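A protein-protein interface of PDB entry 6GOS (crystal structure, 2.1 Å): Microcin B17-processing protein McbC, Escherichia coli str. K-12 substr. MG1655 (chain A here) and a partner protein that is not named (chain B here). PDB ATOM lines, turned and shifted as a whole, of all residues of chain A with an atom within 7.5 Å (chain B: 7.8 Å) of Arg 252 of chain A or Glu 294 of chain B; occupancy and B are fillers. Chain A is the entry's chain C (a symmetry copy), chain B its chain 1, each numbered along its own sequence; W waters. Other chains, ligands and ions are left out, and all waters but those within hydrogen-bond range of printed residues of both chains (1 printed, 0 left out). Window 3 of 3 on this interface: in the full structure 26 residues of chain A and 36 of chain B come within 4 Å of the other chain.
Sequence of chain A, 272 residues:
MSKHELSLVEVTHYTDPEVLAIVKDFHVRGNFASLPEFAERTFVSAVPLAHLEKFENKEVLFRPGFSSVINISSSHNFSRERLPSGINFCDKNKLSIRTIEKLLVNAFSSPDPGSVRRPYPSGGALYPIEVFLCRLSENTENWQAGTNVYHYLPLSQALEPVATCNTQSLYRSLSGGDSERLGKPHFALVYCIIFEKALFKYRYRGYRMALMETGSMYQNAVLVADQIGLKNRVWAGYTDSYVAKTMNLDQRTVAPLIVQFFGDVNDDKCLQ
Among the printed residues, pairs that only touch across the chains: Lys 24 of chain A with Ile 285 of chain B (3.4 Å), Asp 250 of chain A with Leu 293 of chain B (3.4 Å), Gln 251 of chain A with His 286 of chain B (3.5 Å), Arg 252 of chain A with His 286 of chain B (3.99 Å), Arg 252 of chain A with Trp 287 of chain B (3.7 Å) and Arg 252 of chain A with Leu 293 of chain B (3.8 Å).
Water W1 lies within hydrogen-bond range of O of His 286 of chain B and NZ of Lys 24 of chain A.
OD2 of Asp 250 of chain A is in salt-bridge range of NH2 of Arg 252 of chain A. The backbone carbonyl oxygen (O) of Arg 252 of chain A lies within hydrogen-bond range of the side-chain amino group (NZ) of Lys 24 of chain A. The side-chain sulfur (SG) of Cys 195 of chain B lies close to the backbone NH (N) of Trp 287 of chain B, at 3.3 Å.
Of the printed residues of chain B, Arg 252 of chain A touches His 286 (3.99 Å), Trp 287 (3.7 Å), Gln 288 (3.2 Å), Cys 290 (3.1 Å), Leu 293 (3.8 Å) and Glu 294 (3.6 Å). Glu 294 of chain B touches just one residue of chain A: Arg 252. Printed residues of chain A within 4 Å of Ile 285 of chain B: Lys 24 (3.4 Å). Of the printed residues of chain A, Leu 293 of chain B touches Asp 250 and Arg 252. Of the printed residues of chain A, Gln 288 of chain B touches Arg 252 (3.2 Å). Printed residues of chain A within 4 Å of His 286 of chain B: Gln 251 (3.5 Å) and Arg 252 (3.99 Å). Of the printed residues of chain A, Cys 290 of chain B touches Arg 252 (3.1 Å).
Of the 13 printed residues of chain A, 4 touch a printed residue of chain B. Of the 13 printed residues of chain B, 7 touch a printed residue of chain A. Hydrophobic or aromatic side chains of chain B within 4 Å of the printed part of chain A: Ile 285, His 286 and Leu 293.
The backbone carbonyl oxygen of Cys 290 of chain B sits at hydrogen-bond distance from the guanidinium group of Arg 252 of chain A (3.1 Å). The side-chain carboxylate (OE2) of Glu 294 of chain B lies within salt-bridge range of the guanidinium group (NH2) of Arg 252 of chain A, at 3.6 Å. The guanidinium group of Arg 252 of chain A is in hydrogen-bond range of the backbone carbonyl oxygen of Gln 288 of chain B, 3.2 Å away.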
ATOM      1  N   LEU A  20      34.674 -22.089 -18.512  1.00  0.00           N
ATOM      2  CA  LEU A  20      33.493 -22.926 -18.321  1.00  0.00           C
ATOM      3  C   LEU A  20      32.417 -22.580 -19.320  1.00  0.00           C
ATOM      4  O   LEU A  20      31.827 -23.477 -19.891  1.00  0.00           O
ATOM      5  CB  LEU A  20      32.920 -22.797 -16.918  1.00  0.00           C
ATOM      6  CG  LEU A  20      31.657 -23.610 -16.616  1.00  0.00           C
ATOM      7  CD1 LEU A  20      31.935 -25.098 -16.666  1.00  0.00           C
ATOM      8  CD2 LEU A  20      31.110 -23.189 -15.262  1.00  0.00           C
ATOM      9  N   LYS A  24      31.087 -25.099 -22.415  1.00  0.00           N
ATOM     10  CA  LYS A  24      29.665 -25.425 -22.527  1.00  0.00           C
ATOM     11  C   LYS A  24      29.066 -24.987 -23.863  1.00  0.00           C
ATOM     12  O   LYS A  24      28.276 -25.706 -24.478  1.00  0.00           O
ATOM     13  CB  LYS A  24      28.873 -24.776 -21.400  1.00  0.00           C
ATOM     14  CG  LYS A  24      29.023 -25.428 -20.033  1.00  0.00           C
ATOM     15  CD  LYS A  24      28.389 -24.477 -19.021  1.00  0.00           C
ATOM     16  CE  LYS A  24      28.138 -25.108 -17.690  1.00  0.00           C
ATOM     17  NZ  LYS A  24      27.119 -24.287 -16.947  1.00  0.00           N
ATOM     18  N   ILE A 194      31.422 -34.074 -15.613  1.00  0.00           N
ATOM     19  CA  ILE A 194      31.173 -32.968 -14.686  1.00  0.00           C
ATOM     20  C   ILE A 194      32.108 -31.883 -15.153  1.00  0.00           C
ATOM     21  O   ILE A 194      33.334 -32.008 -15.002  1.00  0.00           O
ATOM     22  CB  ILE A 194      31.462 -33.341 -13.223  1.00  0.00           C
ATOM     23  CG1 ILE A 194      30.543 -34.481 -12.772  1.00  0.00           C
ATOM     24  CG2 ILE A 194      31.228 -32.137 -12.300  1.00  0.00           C
ATOM     25  CD1 ILE A 194      30.902 -35.001 -11.394  1.00  0.00           C
ATOM     26  N   PHE A 195      31.537 -30.824 -15.731  1.00  0.00           N
ATOM     27  CA  PHE A 195      32.335 -29.823 -16.465  1.00  0.00           C
ATOM     28  C   PHE A 195      33.426 -29.237 -15.574  1.00  0.00           C
ATOM     29  O   PHE A 195      34.588 -29.209 -15.948  1.00  0.00           O
ATOM     30  CB  PHE A 195      31.481 -28.674 -17.018  1.00  0.00           C
ATOM     31  CG  PHE A 195      30.536 -29.081 -18.119  1.00  0.00           C
ATOM     32  CD1 PHE A 195      31.009 -29.339 -19.405  1.00  0.00           C
ATOM     33  CD2 PHE A 195      29.176 -29.199 -17.875  1.00  0.00           C
ATOM     34  CE1 PHE A 195      30.135 -29.709 -20.433  1.00  0.00           C
ATOM     35  CE2 PHE A 195      28.299 -29.572 -18.898  1.00  0.00           C
ATOM     36  CZ  PHE A 195      28.784 -29.833 -20.175  1.00  0.00           C
ATOM     37  N   GLU A 196      33.042 -28.777 -14.396  1.00  0.00           N
ATOM     38  CA  GLU A 196      34.008 -28.085 -13.536  1.00  0.00           C
ATOM     39  C   GLU A 196      35.103 -28.998 -13.008  1.00  0.00           C
ATOM     40  O   GLU A 196      36.242 -28.566 -12.819  1.00  0.00           O
ATOM     41  CB  GLU A 196      33.304 -27.300 -12.414  1.00  0.00           C
ATOM     42  CG  GLU A 196      32.602 -26.057 -12.962  1.00  0.00           C
ATOM     43  CD  GLU A 196      32.035 -25.145 -11.883  1.00  0.00           C
ATOM     44  OE1 GLU A 196      32.805 -24.760 -10.979  1.00  0.00           O
ATOM     45  OE2 GLU A 196      30.822 -24.791 -11.958  1.00  0.00           O
ATOM     46  N   LYS A 245      17.449 -34.878 -18.143  1.00  0.00           N
ATOM     47  CA  LYS A 245      16.225 -34.594 -17.398  1.00  0.00           C
ATOM     48  C   LYS A 245      15.653 -35.876 -16.803  1.00  0.00           C
ATOM     49  O   LYS A 245      15.212 -35.870 -15.646  1.00  0.00           O
ATOM     50  CB  LYS A 245      15.178 -33.953 -18.322  1.00  0.00           C
ATOM     51  CG  LYS A 245      13.855 -33.512 -17.693  1.00  0.00           C
ATOM     52  CD  LYS A 245      13.895 -32.058 -17.234  1.00  0.00           C
ATOM     53  N   LEU A 249      19.585 -35.262 -13.746  1.00  0.00           N
ATOM     54  CA  LEU A 249      20.860 -34.556 -13.777  1.00  0.00           C
ATOM     55  C   LEU A 249      20.660 -33.042 -14.000  1.00  0.00           C
ATOM     56  O   LEU A 249      19.744 -32.602 -14.700  1.00  0.00           O
ATOM     57  CB  LEU A 249      21.750 -35.117 -14.881  1.00  0.00           C
ATOM     58  CG  LEU A 249      22.105 -36.601 -14.835  1.00  0.00           C
ATOM     59  CD1 LEU A 249      22.993 -36.926 -16.034  1.00  0.00           C
ATOM     60  CD2 LEU A 249      22.814 -36.958 -13.541  1.00  0.00           C
ATOM     61  N   ASP A 250      21.548 -32.263 -13.407  1.00  0.00           N
ATOM     62  CA  ASP A 250      21.566 -30.842 -13.587  1.00  0.00           C
ATOM     63  C   ASP A 250      22.513 -30.499 -14.734  1.00  0.00           C
ATOM     64  O   ASP A 250      23.739 -30.594 -14.598  1.00  0.00           O
ATOM     65  CB  ASP A 250      21.999 -30.171 -12.295  1.00  0.00           C
ATOM     66  CG  ASP A 250      21.772 -28.679 -12.319  1.00  0.00           C
ATOM     67  OD1 ASP A 250      21.959 -28.068 -13.410  1.00  0.00           O
ATOM     68  OD2 ASP A 250      21.445 -28.111 -11.234  1.00  0.00           O
ATOM     69  N   GLN A 251      21.930 -30.086 -15.866  1.00  0.00           N
ATOM     70  CA  GLN A 251      22.697 -29.790 -17.089  1.00  0.00           C
ATOM     71  C   GLN A 251      23.681 -28.631 -16.943  1.00  0.00           C
ATOM     72  O   GLN A 251      24.632 -28.542 -17.694  1.00  0.00           O
ATOM     73  CB  GLN A 251      21.758 -29.587 -18.283  1.00  0.00           C
ATOM     74  CG  GLN A 251      21.055 -30.875 -18.692  1.00  0.00           C
ATOM     75  CD  GLN A 251      20.082 -30.665 -19.819  1.00  0.00           C
ATOM     76  OE1 GLN A 251      20.480 -30.579 -20.961  1.00  0.00           O
ATOM     77  NE2 GLN A 251      18.808 -30.561 -19.498  1.00  0.00           N
ATOM     78  N   ARG A 252      23.514 -27.789 -15.923  1.00  0.00           N
ATOM     79  CA  ARG A 252      24.529 -26.768 -15.617  1.00  0.00           C
ATOM     80  C   ARG A 252      25.866 -27.341 -15.127  1.00  0.00           C
ATOM     81  O   ARG A 252      26.916 -26.738 -15.326  1.00  0.00           O
ATOM     82  CB  ARG A 252      23.967 -25.731 -14.666  1.00  0.00           C
ATOM     83  CG  ARG A 252      22.826 -24.928 -15.290  1.00  0.00           C
ATOM     84  CD  ARG A 252      21.982 -24.173 -14.271  1.00  0.00           C
ATOM     85  NE  ARG A 252      21.445 -25.070 -13.245  1.00  0.00           N
ATOM     86  CZ  ARG A 252      20.805 -24.674 -12.146  1.00  0.00           C
ATOM     87  NH1 ARG A 252      20.557 -23.390 -11.914  1.00  0.00           N
ATOM     88  NH2 ARG A 252      20.384 -25.574 -11.271  1.00  0.00           N
ATOM     89  N   THR A 253      25.824 -28.535 -14.544  1.00  0.00           N
ATOM     90  CA  THR A 253      26.986 -29.172 -13.954  1.00  0.00           C
ATOM     91  C   THR A 253      27.492 -30.384 -14.714  1.00  0.00           C
ATOM     92  O   THR A 253      28.710 -30.594 -14.790  1.00  0.00           O
ATOM     93  CB  THR A 253      26.586 -29.620 -12.542  1.00  0.00           C
ATOM     94  OG1 THR A 253      26.346 -28.447 -11.756  1.00  0.00           O
ATOM     95  CG2 THR A 253      27.638 -30.450 -11.873  1.00  0.00           C
ATOM     96  N   VAL A 254      26.566 -31.207 -15.213  1.00  0.00           N
ATOM     97  CA  VAL A 254      26.894 -32.534 -15.713  1.00  0.00           C
ATOM     98  C   VAL A 254      26.151 -32.797 -17.014  1.00  0.00           C
ATOM     99  O   VAL A 254      25.038 -32.349 -17.175  1.00  0.00           O
ATOM    100  CB  VAL A 254      26.619 -33.623 -14.641  1.00  0.00           C
ATOM    101  CG1 VAL A 254      25.166 -33.614 -14.165  1.00  0.00           C
ATOM    102  CG2 VAL A 254      27.014 -34.998 -15.143  1.00  0.00           C
ATOM    103  N   ALA A 255      26.800 -33.467 -17.968  1.00  0.00           N
ATOM    104  CA  ALA A 255      26.149 -33.812 -19.221  1.00  0.00           C
ATOM    105  C   ALA A 255      26.528 -35.216 -19.659  1.00  0.00           C
ATOM    106  O   ALA A 255      27.654 -35.632 -19.473  1.00  0.00           O
ATOM    107  CB  ALA A 255      26.455 -32.791 -20.327  1.00  0.00           C
ATOM    108  N   TYR B 184      11.519 -24.414 -25.942  1.00  0.00           N
ATOM    109  CA  TYR B 184      11.540 -24.679 -24.518  1.00  0.00           C
ATOM    110  C   TYR B 184      10.534 -25.779 -24.234  1.00  0.00           C
ATOM    111  O   TYR B 184       9.322 -25.560 -24.341  1.00  0.00           O
ATOM    112  CB  TYR B 184      11.172 -23.415 -23.721  1.00  0.00           C
ATOM    113  CG  TYR B 184      11.023 -23.656 -22.230  1.00  0.00           C
ATOM    114  CD1 TYR B 184      11.875 -24.538 -21.542  1.00  0.00           C
ATOM    115  CD2 TYR B 184      10.038 -23.015 -21.513  1.00  0.00           C
ATOM    116  CE1 TYR B 184      11.701 -24.785 -20.187  1.00  0.00           C
ATOM    117  CE2 TYR B 184       9.875 -23.238 -20.157  1.00  0.00           C
ATOM    118  CZ  TYR B 184      10.708 -24.114 -19.501  1.00  0.00           C
ATOM    119  OH  TYR B 184      10.521 -24.323 -18.165  1.00  0.00           O
ATOM    120  N   CYS B 195      17.038 -18.199 -20.465  1.00  0.00           N
ATOM    121  CA  CYS B 195      18.353 -18.701 -20.800  1.00  0.00           C
ATOM    122  C   CYS B 195      18.850 -18.036 -22.083  1.00  0.00           C
ATOM    123  O   CYS B 195      20.038 -17.764 -22.218  1.00  0.00           O
ATOM    124  CB  CYS B 195      18.329 -20.228 -20.953  1.00  0.00           C
ATOM    125  SG  CYS B 195      18.130 -21.172 -19.416  1.00  0.00           S
ATOM    126  N   ILE B 285      23.133 -22.483 -24.197  1.00  0.00           N
ATOM    127  CA  ILE B 285      23.229 -23.241 -22.959  1.00  0.00           C
ATOM    128  C   ILE B 285      22.200 -22.761 -21.929  1.00  0.00           C
ATOM    129  O   ILE B 285      21.659 -21.653 -22.040  1.00  0.00           O
ATOM    130  CB  ILE B 285      24.646 -23.221 -22.347  1.00  0.00           C
ATOM    131  CG1 ILE B 285      25.123 -21.793 -21.980  1.00  0.00           C
ATOM    132  CG2 ILE B 285      25.627 -23.908 -23.292  1.00  0.00           C
ATOM    133  CD1 ILE B 285      26.391 -21.793 -21.160  1.00  0.00           C
ATOM    134  N   HIS B 286      21.922 -23.621 -20.950  1.00  0.00           N
ATOM    135  CA  HIS B 286      21.202 -23.199 -19.741  1.00  0.00           C
ATOM    136  C   HIS B 286      22.021 -22.116 -19.033  1.00  0.00           C
ATOM    137  O   HIS B 286      23.202 -22.315 -18.745  1.00  0.00           O
ATOM    138  CB  HIS B 286      20.969 -24.387 -18.777  1.00  0.00           C
ATOM    139  CG  HIS B 286      20.019 -25.417 -19.305  1.00  0.00           C
ATOM    140  ND1 HIS B 286      20.444 -26.528 -20.006  1.00  0.00           N
ATOM    141  CD2 HIS B 286      18.660 -25.468 -19.297  1.00  0.00           C
ATOM    142  CE1 HIS B 286      19.387 -27.239 -20.374  1.00  0.00           C
ATOM    143  NE2 HIS B 286      18.293 -26.616 -19.963  1.00  0.00           N
ATOM    144  N   TRP B 287      21.403 -20.970 -18.803  1.00  0.00           N
ATOM    145  CA  TRP B 287      21.966 -19.927 -17.988  1.00  0.00           C
ATOM    146  C   TRP B 287      22.112 -20.360 -16.526  1.00  0.00           C
ATOM    147  O   TRP B 287      21.196 -20.911 -15.916  1.00  0.00           O
ATOM    148  CB  TRP B 287      21.106 -18.681 -18.075  1.00  0.00           C
ATOM    149  CG  TRP B 287      21.655 -17.512 -17.332  1.00  0.00           C
ATOM    150  CD1 TRP B 287      22.948 -17.105 -17.304  1.00  0.00           C
ATOM    151  CD2 TRP B 287      20.913 -16.572 -16.537  1.00  0.00           C
ATOM    152  NE1 TRP B 287      23.064 -15.964 -16.550  1.00  0.00           N
ATOM    153  CE2 TRP B 287      21.830 -15.617 -16.065  1.00  0.00           C
ATOM    154  CE3 TRP B 287      19.559 -16.429 -16.209  1.00  0.00           C
ATOM    155  CZ2 TRP B 287      21.451 -14.548 -15.253  1.00  0.00           C
ATOM    156  CZ3 TRP B 287      19.169 -15.346 -15.394  1.00  0.00           C
ATOM    157  CH2 TRP B 287      20.120 -14.425 -14.930  1.00  0.00           C
ATOM    158  N   GLN B 288      23.295 -20.118 -15.982  1.00  0.00           N
ATOM    159  CA  GLN B 288      23.631 -20.593 -14.660  1.00  0.00           C
ATOM    160  C   GLN B 288      22.647 -20.116 -13.571  1.00  0.00           C
ATOM    161  O   GLN B 288      22.352 -20.884 -12.648  1.00  0.00           O
ATOM    162  CB  GLN B 288      25.089 -20.239 -14.316  1.00  0.00           C
ATOM    163  CG  GLN B 288      25.431 -18.750 -14.255  1.00  0.00           C
ATOM    164  CD  GLN B 288      26.930 -18.494 -14.342  1.00  0.00           C
ATOM    165  OE1 GLN B 288      27.780 -19.341 -13.962  1.00  0.00           O
ATOM    166  NE2 GLN B 288      27.272 -17.334 -14.880  1.00  0.00           N
ATOM    167  N   ALA B 289      22.147 -18.882 -13.697  1.00  0.00           N
ATOM    168  CA  ALA B 289      21.313 -18.286 -12.670  1.00  0.00           C
ATOM    169  C   ALA B 289      19.815 -18.488 -12.910  1.00  0.00           C
ATOM    170  O   ALA B 289      19.013 -17.888 -12.206  1.00  0.00           O
ATOM    171  CB  ALA B 289      21.622 -16.802 -12.517  1.00  0.00           C
ATOM    172  N   CYS B 290      19.459 -19.301 -13.904  1.00  0.00           N
ATOM    173  CA  CYS B 290      18.073 -19.591 -14.236  1.00  0.00           C
ATOM    174  C   CYS B 290      17.695 -20.886 -13.565  1.00  0.00           C
ATOM    175  O   CYS B 290      18.484 -21.824 -13.535  1.00  0.00           O
ATOM    176  CB  CYS B 290      17.898 -19.807 -15.747  1.00  0.00           C
ATOM    177  SG  CYS B 290      16.196 -19.796 -16.318  1.00  0.00           S
ATOM    178  N   SER B 291      16.455 -20.973 -13.135  1.00  0.00           N
ATOM    179  CA  SER B 291      15.970 -22.188 -12.485  1.00  0.00           C
ATOM    180  C   SER B 291      14.961 -22.959 -13.339  1.00  0.00           C
ATOM    181  O   SER B 291      14.251 -23.815 -12.808  1.00  0.00           O
ATOM    182  CB  SER B 291      15.354 -21.809 -11.153  1.00  0.00           C
ATOM    183  OG  SER B 291      14.368 -20.816 -11.412  1.00  0.00           O
ATOM    184  N   CYS B 292      14.942 -22.738 -14.655  1.00  0.00           N
ATOM    185  CA  CYS B 292      14.028 -23.507 -15.505  1.00  0.00           C
ATOM    186  C   CYS B 292      14.230 -25.013 -15.384  1.00  0.00           C
ATOM    187  O   CYS B 292      13.267 -25.755 -15.383  1.00  0.00           O
ATOM    188  CB  CYS B 292      14.057 -23.085 -16.988  1.00  0.00           C
ATOM    189  SG  CYS B 292      15.624 -23.212 -17.905  1.00  0.00           S
ATOM    190  N   LEU B 293      15.461 -25.474 -15.252  1.00  0.00           N
ATOM    191  CA  LEU B 293      15.686 -26.917 -15.194  1.00  0.00           C
ATOM    192  C   LEU B 293      15.451 -27.511 -13.779  1.00  0.00           C
ATOM    193  O   LEU B 293      15.466 -28.736 -13.606  1.00  0.00           O
ATOM    194  CB  LEU B 293      17.060 -27.278 -15.789  1.00  0.00           C
ATOM    195  CG  LEU B 293      18.333 -26.840 -15.049  1.00  0.00           C
ATOM    196  CD1 LEU B 293      18.654 -27.802 -13.908  1.00  0.00           C
ATOM    197  CD2 LEU B 293      19.491 -26.776 -16.036  1.00  0.00           C
ATOM    198  N   GLU B 294      15.258 -26.643 -12.784  1.00  0.00           N
ATOM    199  CA  GLU B 294      14.876 -27.067 -11.443  1.00  0.00           C
ATOM    200  C   GLU B 294      13.369 -27.325 -11.339  1.00  0.00           C
ATOM    201  O   GLU B 294      12.937 -28.048 -10.466  1.00  0.00           O
ATOM    202  CB  GLU B 294      15.296 -26.024 -10.399  1.00  0.00           C
ATOM    203  CG  GLU B 294      16.788 -25.735 -10.404  1.00  0.00           C
ATOM    204  CD  GLU B 294      17.247 -24.942  -9.181  1.00  0.00           C
ATOM    205  OE1 GLU B 294      16.696 -23.845  -8.912  1.00  0.00           O
ATOM    206  OE2 GLU B 294      18.172 -25.427  -8.491  1.00  0.00           O
ATOM    207  N   ARG B 295      12.571 -26.730 -12.221  1.00  0.00           N
ATOM    208  CA  ARG B 295      11.113 -26.891 -12.147  1.00  0.00           C
ATOM    209  C   ARG B 295      10.686 -28.300 -12.600  1.00  0.00           C
ATOM    210  O   ARG B 295      11.423 -29.006 -13.278  1.00  0.00           O
ATOM    211  CB  ARG B 295      10.384 -25.715 -12.858  1.00  0.00           C
ATOM    212  CG  ARG B 295      10.626 -24.410 -12.067  1.00  0.00           C
ATOM    213  CD  ARG B 295       9.661 -23.256 -12.317  1.00  0.00           C
ATOM    214  NE  ARG B 295       9.788 -22.702 -13.661  1.00  0.00           N
ATOM    215  CZ  ARG B 295      10.764 -21.892 -14.102  1.00  0.00           C
ATOM    216  NH1 ARG B 295      11.735 -21.470 -13.295  1.00  0.00           N
ATOM    217  NH2 ARG B 295      10.763 -21.478 -15.382  1.00  0.00           N
ATOM    218  OXT ARG B 295       9.643 -28.815 -12.204  1.00  0.00           O
HETATM  219  O   HOH W   1      24.717 -24.430 -18.378  1.00  0.00           O
